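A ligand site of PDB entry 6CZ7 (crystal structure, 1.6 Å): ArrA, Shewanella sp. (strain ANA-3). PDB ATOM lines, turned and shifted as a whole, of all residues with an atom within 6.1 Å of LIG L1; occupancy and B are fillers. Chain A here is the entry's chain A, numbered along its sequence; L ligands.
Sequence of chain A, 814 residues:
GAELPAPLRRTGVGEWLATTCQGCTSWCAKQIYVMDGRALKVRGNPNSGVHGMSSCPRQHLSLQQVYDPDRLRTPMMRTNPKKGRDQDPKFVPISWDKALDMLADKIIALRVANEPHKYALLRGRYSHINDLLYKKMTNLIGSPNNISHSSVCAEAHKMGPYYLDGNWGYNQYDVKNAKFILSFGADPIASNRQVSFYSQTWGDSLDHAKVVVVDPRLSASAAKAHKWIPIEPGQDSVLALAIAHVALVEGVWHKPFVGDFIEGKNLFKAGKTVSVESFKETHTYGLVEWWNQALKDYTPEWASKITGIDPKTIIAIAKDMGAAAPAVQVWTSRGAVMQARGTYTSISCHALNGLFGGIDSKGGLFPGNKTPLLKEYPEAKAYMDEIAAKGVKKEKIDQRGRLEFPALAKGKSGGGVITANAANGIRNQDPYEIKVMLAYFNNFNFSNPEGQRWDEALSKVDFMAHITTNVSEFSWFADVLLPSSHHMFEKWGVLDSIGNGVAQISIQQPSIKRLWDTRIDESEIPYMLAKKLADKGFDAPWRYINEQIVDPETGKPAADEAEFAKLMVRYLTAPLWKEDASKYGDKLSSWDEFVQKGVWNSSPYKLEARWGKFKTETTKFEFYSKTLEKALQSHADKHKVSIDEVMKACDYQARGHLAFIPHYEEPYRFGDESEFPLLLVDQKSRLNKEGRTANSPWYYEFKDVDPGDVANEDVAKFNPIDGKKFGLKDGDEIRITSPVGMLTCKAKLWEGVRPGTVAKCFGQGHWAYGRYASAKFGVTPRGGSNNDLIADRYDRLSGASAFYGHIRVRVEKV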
ATOM      1  N   CYS A  21      24.902  -5.050 -33.721  1.00  0.00           N
ATOM      2  CA  CYS A  21      23.901  -4.524 -32.814  1.00  0.00           C
ATOM      3  C   CYS A  21      24.560  -3.531 -31.862  1.00  0.00           C
ATOM      4  O   CYS A  21      25.734  -3.667 -31.496  1.00  0.00           O
ATOM      5  CB  CYS A  21      23.268  -5.669 -32.031  1.00  0.00           C
ATOM      6  SG  CYS A  21      21.866  -5.193 -31.027  1.00  0.00           S
ATOM      7  N   GLN A  22      23.802  -2.511 -31.458  1.00  0.00           N
ATOM      8  CA  GLN A  22      24.319  -1.566 -30.473  1.00  0.00           C
ATOM      9  C   GLN A  22      23.305  -1.303 -29.375  1.00  0.00           C
ATOM     10  O   GLN A  22      23.289  -0.215 -28.783  1.00  0.00           O
ATOM     11  CB  GLN A  22      24.735  -0.264 -31.139  1.00  0.00           C
ATOM     12  CG  GLN A  22      25.891  -0.435 -32.087  1.00  0.00           C
ATOM     13  CD  GLN A  22      26.456   0.887 -32.506  1.00  0.00           C
ATOM     14  OE1 GLN A  22      26.104   1.416 -33.556  1.00  0.00           O
ATOM     15  NE2 GLN A  22      27.322   1.448 -31.676  1.00  0.00           N
ATOM     16  N   GLY A  23      22.459  -2.287 -29.098  1.00  0.00           N
ATOM     17  CA  GLY A  23      21.552  -2.215 -27.959  1.00  0.00           C
ATOM     18  C   GLY A  23      22.281  -2.059 -26.649  1.00  0.00           C
ATOM     19  O   GLY A  23      21.690  -1.588 -25.676  1.00  0.00           O
ATOM     20  N   CYS A  24      23.537  -2.463 -26.605  1.00  0.00           N
ATOM     21  CA  CYS A  24      24.435  -2.098 -25.530  1.00  0.00           C
ATOM     22  C   CYS A  24      25.860  -2.159 -26.071  1.00  0.00           C
ATOM     23  O   CYS A  24      26.101  -2.557 -27.218  1.00  0.00           O
ATOM     24  CB  CYS A  24      24.273  -3.004 -24.295  1.00  0.00           C
ATOM     25  SG  CYS A  24      24.512  -4.757 -24.527  1.00  0.00           S
ATOM     26  N   THR A  25      26.802  -1.802 -25.222  1.00  0.00           N
ATOM     27  CA  THR A  25      28.209  -1.763 -25.599  1.00  0.00           C
ATOM     28  C   THR A  25      28.829  -3.152 -25.649  1.00  0.00           C
ATOM     29  O   THR A  25      30.051  -3.271 -25.780  1.00  0.00           O
ATOM     30  CB  THR A  25      28.933  -0.852 -24.624  1.00  0.00           C
ATOM     31  OG1 THR A  25      28.552  -1.218 -23.296  1.00  0.00           O
ATOM     32  CG2 THR A  25      28.550   0.612 -24.879  1.00  0.00           C
ATOM     33  N   SER A  26      28.005  -4.198 -25.527  1.00  0.00           N
ATOM     34  CA  SER A  26      28.420  -5.508 -25.986  1.00  0.00           C
ATOM     35  C   SER A  26      28.753  -5.476 -27.465  1.00  0.00           C
ATOM     36  O   SER A  26      29.652  -6.190 -27.919  1.00  0.00           O
ATOM     37  CB  SER A  26      27.320  -6.531 -25.724  1.00  0.00           C
ATOM     38  OG  SER A  26      27.028  -6.648 -24.346  1.00  0.00           O
ATOM     39  N   TRP A  27      28.029  -4.660 -28.227  1.00  0.00           N
ATOM     40  CA  TRP A  27      28.245  -4.456 -29.648  1.00  0.00           C
ATOM     41  C   TRP A  27      28.430  -5.784 -30.383  1.00  0.00           C
ATOM     42  O   TRP A  27      29.417  -6.027 -31.068  1.00  0.00           O
ATOM     43  CB  TRP A  27      29.439  -3.531 -29.870  1.00  0.00           C
ATOM     44  CG  TRP A  27      29.161  -2.107 -29.471  1.00  0.00           C
ATOM     45  CD1 TRP A  27      27.935  -1.532 -29.265  1.00  0.00           C
ATOM     46  CD2 TRP A  27      30.124  -1.082 -29.241  1.00  0.00           C
ATOM     47  NE1 TRP A  27      28.080  -0.212 -28.913  1.00  0.00           N
ATOM     48  CE2 TRP A  27      29.426   0.087 -28.889  1.00  0.00           C
ATOM     49  CE3 TRP A  27      31.520  -1.047 -29.292  1.00  0.00           C
ATOM     50  CZ2 TRP A  27      30.072   1.286 -28.588  1.00  0.00           C
ATOM     51  CZ3 TRP A  27      32.165   0.140 -28.983  1.00  0.00           C
ATOM     52  CH2 TRP A  27      31.444   1.284 -28.647  1.00  0.00           C
ATOM     53  N   CYS A  28      27.410  -6.633 -30.249  1.00  0.00           N
ATOM     54  CA  CYS A  28      27.479  -7.963 -30.831  1.00  0.00           C
ATOM     55  C   CYS A  28      27.470  -7.928 -32.345  1.00  0.00           C
ATOM     56  O   CYS A  28      26.694  -7.186 -32.969  1.00  0.00           O
ATOM     57  CB  CYS A  28      26.316  -8.819 -30.360  1.00  0.00           C
ATOM     58  SG  CYS A  28      26.284  -9.096 -28.599  1.00  0.00           S
ATOM     59  N   LYS A  30      26.251  -9.378 -35.692  1.00  0.00           N
ATOM     60  CA  LYS A  30      24.967  -9.948 -36.018  1.00  0.00           C
ATOM     61  C   LYS A  30      24.908 -10.350 -37.479  1.00  0.00           C
ATOM     62  O   LYS A  30      25.710  -9.905 -38.306  1.00  0.00           O
ATOM     63  CB  LYS A  30      23.823  -8.948 -35.767  1.00  0.00           C
ATOM     64  CG  LYS A  30      23.691  -8.525 -34.341  1.00  0.00           C
ATOM     65  CD  LYS A  30      23.396  -9.740 -33.495  1.00  0.00           C
ATOM     66  CE  LYS A  30      22.848  -9.372 -32.136  1.00  0.00           C
ATOM     67  NZ  LYS A  30      22.582 -10.582 -31.330  1.00  0.00           N
ATOM     68  N   SER A  55      23.009 -14.722 -28.279  1.00  0.00           N
ATOM     69  CA  SER A  55      22.485 -13.379 -28.240  1.00  0.00           C
ATOM     70  C   SER A  55      21.621 -13.177 -27.003  1.00  0.00           C
ATOM     71  O   SER A  55      20.955 -14.104 -26.522  1.00  0.00           O
ATOM     72  CB  SER A  55      21.611 -13.070 -29.462  1.00  0.00           C
ATOM     73  OG  SER A  55      21.126 -11.751 -29.419  1.00  0.00           O
ATOM     74  N   CYS A  56      21.593 -11.944 -26.514  1.00  0.00           N
ATOM     75  CA  CYS A  56      20.586 -11.520 -25.556  1.00  0.00           C
ATOM     76  C   CYS A  56      19.268 -11.311 -26.273  1.00  0.00           C
ATOM     77  O   CYS A  56      19.193 -11.318 -27.509  1.00  0.00           O
ATOM     78  CB  CYS A  56      21.057 -10.273 -24.825  1.00  0.00           C
ATOM     79  SG  CYS A  56      20.409  -8.731 -25.459  1.00  0.00           S
ATOM     80  N   PRO A  57      18.181 -11.094 -25.520  1.00  0.00           N
ATOM     81  CA  PRO A  57      16.851 -11.066 -26.151  1.00  0.00           C
ATOM     82  C   PRO A  57      16.588  -9.813 -26.972  1.00  0.00           C
ATOM     83  O   PRO A  57      15.683  -9.816 -27.809  1.00  0.00           O
ATOM     84  CB  PRO A  57      15.895 -11.156 -24.953  1.00  0.00           C
ATOM     85  CG  PRO A  57      16.675 -10.496 -23.826  1.00  0.00           C
ATOM     86  CD  PRO A  57      18.112 -10.929 -24.056  1.00  0.00           C
ATOM     87  N   ARG A  58      17.354  -8.742 -26.740  1.00  0.00           N
ATOM     88  CA  ARG A  58      17.068  -7.466 -27.362  1.00  0.00           C
ATOM     89  C   ARG A  58      17.379  -7.460 -28.856  1.00  0.00           C
ATOM     90  O   ARG A  58      16.935  -6.534 -29.558  1.00  0.00           O
ATOM     91  CB  ARG A  58      17.859  -6.361 -26.664  1.00  0.00           C
ATOM     92  CG  ARG A  58      17.308  -6.026 -25.291  1.00  0.00           C
ATOM     93  CD  ARG A  58      18.245  -5.158 -24.491  1.00  0.00           C
ATOM     94  NE  ARG A  58      19.405  -5.924 -24.091  1.00  0.00           N
ATOM     95  CZ  ARG A  58      20.620  -5.406 -23.928  1.00  0.00           C
ATOM     96  NH1 ARG A  58      20.829  -4.105 -24.112  1.00  0.00           N
ATOM     97  NH2 ARG A  58      21.616  -6.190 -23.581  1.00  0.00           N
ATOM     98  N   GLN A  59      18.116  -8.447 -29.364  1.00  0.00           N
ATOM     99  CA  GLN A  59      18.399  -8.432 -30.794  1.00  0.00           C
ATOM    100  C   GLN A  59      17.098  -8.372 -31.593  1.00  0.00           C
ATOM    101  O   GLN A  59      17.045  -7.732 -32.645  1.00  0.00           O
ATOM    102  CB  GLN A  59      19.234  -9.633 -31.195  1.00  0.00           C
ATOM    103  CG  GLN A  59      18.568 -10.983 -31.098  1.00  0.00           C
ATOM    104  CD  GLN A  59      19.435 -12.089 -31.674  1.00  0.00           C
ATOM    105  OE1 GLN A  59      20.376 -11.831 -32.439  1.00  0.00           O
ATOM    106  NE2 GLN A  59      19.126 -13.317 -31.310  1.00  0.00           N
ATOM    107  N   SER A  62      15.352  -4.945 -32.212  1.00  0.00           N
ATOM    108  CA  SER A  62      15.932  -4.147 -33.280  1.00  0.00           C
ATOM    109  C   SER A  62      14.961  -3.967 -34.436  1.00  0.00           C
ATOM    110  O   SER A  62      14.948  -2.921 -35.088  1.00  0.00           O
ATOM    111  CB  SER A  62      17.194  -4.811 -33.811  1.00  0.00           C
ATOM    112  OG  SER A  62      18.046  -5.208 -32.749  1.00  0.00           O
ATOM    113  N   ASN A 192      25.508  -5.049 -18.493  1.00  0.00           N
ATOM    114  CA  ASN A 192      26.964  -5.098 -18.654  1.00  0.00           C
ATOM    115  C   ASN A 192      27.303  -5.419 -20.113  1.00  0.00           C
ATOM    116  O   ASN A 192      26.437  -5.273 -20.992  1.00  0.00           O
ATOM    117  CB  ASN A 192      27.601  -6.094 -17.683  1.00  0.00           C
ATOM    118  CG  ASN A 192      29.033  -5.706 -17.325  1.00  0.00           C
ATOM    119  OD1 ASN A 192      29.963  -6.025 -18.066  1.00  0.00           O
ATOM    120  ND2 ASN A 192      29.213  -5.018 -16.205  1.00  0.00           N
ATOM    121  N   GLN A 194      28.858  -7.940 -22.235  1.00  0.00           N
ATOM    122  CA  GLN A 194      28.715  -8.993 -23.237  1.00  0.00           C
ATOM    123  C   GLN A 194      27.551  -9.864 -22.789  1.00  0.00           C
ATOM    124  O   GLN A 194      27.731 -11.010 -22.364  1.00  0.00           O
ATOM    125  CB  GLN A 194      29.998  -9.773 -23.414  1.00  0.00           C
ATOM    126  CG  GLN A 194      30.440  -9.763 -24.877  1.00  0.00           C
ATOM    127  CD  GLN A 194      29.307 -10.089 -25.849  1.00  0.00           C
ATOM    128  OE1 GLN A 194      28.396 -10.870 -25.540  1.00  0.00           O
ATOM    129  NE2 GLN A 194      29.330  -9.462 -27.017  1.00  0.00           N
ATOM    130  N   VAL A 195      26.335  -9.314 -22.865  1.00  0.00           N
ATOM    131  CA  VAL A 195      25.184 -10.037 -22.346  1.00  0.00           C
ATOM    132  C   VAL A 195      25.038 -11.361 -23.077  1.00  0.00           C
ATOM    133  O   VAL A 195      24.670 -12.377 -22.475  1.00  0.00           O
ATOM    134  CB  VAL A 195      23.909  -9.180 -22.450  1.00  0.00           C
ATOM    135  CG1 VAL A 195      22.773  -9.904 -21.737  1.00  0.00           C
ATOM    136  CG2 VAL A 195      24.164  -7.821 -21.836  1.00  0.00           C
ATOM    137  N   SER A 196      25.343 -11.373 -24.380  1.00  0.00           N
ATOM    138  CA  SER A 196      25.244 -12.585 -25.170  1.00  0.00           C
ATOM    139  C   SER A 196      26.195 -13.647 -24.645  1.00  0.00           C
ATOM    140  O   SER A 196      25.789 -14.787 -24.375  1.00  0.00           O
ATOM    141  CB  SER A 196      25.528 -12.267 -26.629  1.00  0.00           C
ATOM    142  OG  SER A 196      24.600 -11.315 -27.126  1.00  0.00           O
ATOM    143  N   ASN A 688      15.995  -2.956 -22.344  1.00  0.00           N
ATOM    144  CA  ASN A 688      16.437  -1.655 -22.817  1.00  0.00           C
ATOM    145  C   ASN A 688      17.582  -1.815 -23.814  1.00  0.00           C
ATOM    146  O   ASN A 688      18.661  -2.292 -23.446  1.00  0.00           O
ATOM    147  CB  ASN A 688      16.993  -0.786 -21.674  1.00  0.00           C
ATOM    148  CG  ASN A 688      15.943  -0.068 -20.880  1.00  0.00           C
ATOM    149  OD1 ASN A 688      14.751  -0.059 -21.221  1.00  0.00           O
ATOM    150  ND2 ASN A 688      16.378   0.558 -19.807  1.00  0.00           N
ATOM    151  N   LYS A 689      17.382  -1.343 -25.041  1.00  0.00           N
ATOM    152  CA  LYS A 689      18.504  -1.033 -25.931  1.00  0.00           C
ATOM    153  C   LYS A 689      18.848   0.424 -25.624  1.00  0.00           C
ATOM    154  O   LYS A 689      18.386   1.362 -26.283  1.00  0.00           O
ATOM    155  CB  LYS A 689      18.146  -1.270 -27.384  1.00  0.00           C
ATOM    156  CG  LYS A 689      17.890  -2.756 -27.677  1.00  0.00           C
ATOM    157  CD  LYS A 689      17.691  -3.022 -29.149  1.00  0.00           C
ATOM    158  CE  LYS A 689      19.030  -3.076 -29.892  1.00  0.00           C
ATOM    159  NZ  LYS A 689      18.875  -3.007 -31.366  1.00  0.00           N
HETATM  160 FE1  LIG L   1      23.610  -5.642 -26.557  1.00  0.00          FE
HETATM  161 FE2  LIG L   1      22.005  -7.772 -26.843  1.00  0.00          FE
HETATM  162 FE3  LIG L   1      24.410  -7.765 -28.036  1.00  0.00          FE
HETATM  163 FE4  LIG L   1      22.494  -6.152 -28.986  1.00  0.00          FE
HETATM  164  S1  LIG L   1      22.440  -8.447 -28.958  1.00  0.00           S
HETATM  165  S2  LIG L   1      24.626  -5.535 -28.559  1.00  0.00           S
HETATM  166  S3  LIG L   1      21.415  -5.565 -27.096  1.00  0.00           S
HETATM  167  S4  LIG L   1      24.036  -7.800 -25.833  1.00  0.00           S
HETATM  168  P1  LG2 L   2      23.924  -1.372 -14.958  1.00  0.00           P
HETATM  169  O1  LG2 L   2      23.400  -2.241 -16.060  1.00  0.00           O
HETATM  170  O2  LG2 L   2      23.881   0.094 -15.248  1.00  0.00           O
HETATM  171  O3  LG2 L   2      25.447  -1.824 -14.529  1.00  0.00           O
HETATM  172  O4  LG2 L   2      26.476  -2.170 -17.074  1.00  0.00           O
HETATM  173  P2  LG2 L   2      26.775  -2.257 -15.462  1.00  0.00           P
HETATM  174  O5  LG2 L   2      27.859  -1.276 -15.069  1.00  0.00           O
HETATM  175  O6  LG2 L   2      27.036  -3.666 -15.031  1.00  0.00           O
HETATM  176  O7  LG2 L   2      23.073  -1.855 -13.628  1.00  0.00           O
HETATM  177  C1  LG2 L   2      23.135  -1.169 -12.405  1.00  0.00           C
HETATM  178  C2  LG2 L   2      22.923  -2.273 -11.384  1.00  0.00           C
HETATM  179  O8  LG2 L   2      23.511  -1.750  -9.966  1.00  0.00           O
HETATM  180  C3  LG2 L   2      21.692  -2.604 -11.151  1.00  0.00           C
HETATM  181  O9  LG2 L   2      21.687  -4.114 -11.024  1.00  0.00           O
HETATM  182  C4  LG2 L   2      21.210  -2.001  -9.816  1.00  0.00           C
HETATM  183  O10 LG2 L   2      20.419  -2.814  -9.096  1.00  0.00           O
HETATM  184  C5  LG2 L   2      22.534  -2.006  -9.098  1.00  0.00           C
HETATM  185  N1  LG2 L   2      22.908  -1.127  -7.982  1.00  0.00           N
HETATM  186  C6  LG2 L   2      22.199   0.023  -7.981  1.00  0.00           C
HETATM  187  N2  LG2 L   2      22.670   0.725  -6.893  1.00  0.00           N
HETATM  188  C7  LG2 L   2      23.656  -0.013  -6.312  1.00  0.00           C
HETATM  189  C8  LG2 L   2      24.637   0.066  -5.123  1.00  0.00           C
HETATM  190  O11 LG2 L   2      24.692   0.975  -4.385  1.00  0.00           O
HETATM  191  N3  LG2 L   2      25.537  -1.034  -4.892  1.00  0.00           N
HETATM  192  C9  LG2 L   2      25.552  -2.172  -5.739  1.00  0.00           C
HETATM  193  N4  LG2 L   2      26.429  -3.296  -5.532  1.00  0.00           N
HETATM  194  N5  LG2 L   2      24.653  -2.265  -6.840  1.00  0.00           N
HETATM  195  C10 LG2 L   2      23.745  -1.139  -7.045  1.00  0.00           C
HETATM  196  C11 LG2 L   2      26.432  -0.888 -17.667  1.00  0.00           C
HETATM  197  C12 LG2 L   2      26.619  -1.079 -19.149  1.00  0.00           C
HETATM  198  O12 LG2 L   2      25.460  -2.079 -19.626  1.00  0.00           O
HETATM  199  C13 LG2 L   2      26.482   0.058 -19.801  1.00  0.00           C
HETATM  200  S1  LG2 L   2      27.529   1.471 -19.349  1.00  0.00           S
HETATM  201  C14 LG2 L   2      25.864   0.076 -21.199  1.00  0.00           C
HETATM  202  S2  LG2 L   2      25.917   1.586 -22.144  1.00  0.00           S
HETATM  203  C15 LG2 L   2      25.126  -1.070 -21.671  1.00  0.00           C
HETATM  204  N6  LG2 L   2      23.655  -0.524 -21.530  1.00  0.00           N
HETATM  205  C16 LG2 L   2      22.721  -1.558 -21.425  1.00  0.00           C
HETATM  206  C17 LG2 L   2      21.282  -1.261 -21.632  1.00  0.00           C
HETATM  207  O13 LG2 L   2      20.901  -0.198 -21.877  1.00  0.00           O
HETATM  208  N7  LG2 L   2      20.335  -2.351 -21.498  1.00  0.00           N
HETATM  209  C18 LG2 L   2      20.815  -3.750 -21.149  1.00  0.00           C
HETATM  210  N8  LG2 L   2      19.870  -4.809 -21.018  1.00  0.00           N
HETATM  211  N9  LG2 L   2      22.231  -4.083 -20.959  1.00  0.00           N
HETATM  212  C19 LG2 L   2      23.175  -3.048 -21.074  1.00  0.00           C
HETATM  213  N10 LG2 L   2      24.473  -3.471 -20.902  1.00  0.00           N
HETATM  214  C20 LG2 L   2      25.509  -2.295 -20.938  1.00  0.00           C
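OG of Ser 196 sits close to S4 of LIG L1 (3.8 Å).
An iron atom (FE2) of LIG L1 is bound by the side-chain sulfur (SG) of Cys 56, at 2.3 Å.
FE3 of LIG L1 is bound by SG of Cys 28 (2.4 Å).
O6 of LG2 L2 is in hydrogen-bond range of ND2 of Asn 192 (2.8 Å).
An oxygen (O12) of LG2 L2 is in hydrogen-bond range of the backbone NH (N) of Asn 192 (3.2 Å).
The side-chain hydroxyl of Ser 55 lies close to a sulfur (S1) of LIG L1, at 3.6 Å.
FE1 of LIG L1 is bound by SG of Cys 24.
S1 of LIG L1 sits close to NZ of Lys 30 (3.2 Å).
SG of Cys 21 is bound to FE4 of LIG L1, 2.3 Å away.
S4 of LIG L1 sits close to OG of Ser 26 (3.5 Å).
The backbone carbonyl oxygen (O) of Asn 192 lies within hydrogen-bond range of a nitrogen (N10) of LG2 L2 (2.7 Å).
A sulfur (S3) of LIG L1 lies close to the guanidinium group (NH1) of Arg 58.
N7 of LG2 L2 sits at hydrogen-bond distance from O of Asn 688, 2.6 Å away.
N of Trp 27 lies close to S2 of LIG L1 (3.5 Å).
NH2 of Arg 58 is in hydrogen-bond range of N9 of LG2 L2, 3.4 Å away.
The backbone NH (N) of Cys 24 lies close to a sulfur (S3) of LIG L1 (3.8 Å).
The backbone NH of Cys 28 lies close to a sulfur (S2) of LIG L1 (3.4 Å).
The side-chain hydroxyl (OG) of Ser 26 sits at hydrogen-bond distance from the backbone NH (N) of Gln 194.
SG of Cys 56 sits close to NE of Arg 58 (3.3 Å).
SG of Cys 21 sits close to NZ of Lys 689, at 3.7 Å.
OE1 of Gln 194 lies close to N of Ser 196, at 3.3 Å.
The side-chain sulfur (SG) of Cys 28 lies close to the side-chain amide nitrogen (NE2) of Gln 194 (3.5 Å).
The indole nitrogen (NE1) of Trp 27 sits close to the side-chain amide nitrogen (NE2) of Gln 22 (3.3 Å).
The side-chain amino group of Lys 30 sits at hydrogen-bond distance from the side-chain hydroxyl of Ser 55 (2.7 Å).
The side-chain hydroxyl of Ser 55 sits close to the side-chain amide oxygen of Gln 59, at 3.1 Å.
Gly 23 touches LIG L1 (CA to S3, 3.5 Å).
Val 195 touches LIG L1.
Hydrophobic or aromatic side chains that line LIG L1: Val 195.
Within 4 Å of LIG L1: Cys 21, Gly 23, Cys 24, Ser 26, Trp 27, Cys 28, Lys 30, Ser 55, Cys 56, Arg 58, Val 195 and Ser 196.
Along chain A the residues within 4 Å of LIG L1 span positions 21 to 196.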
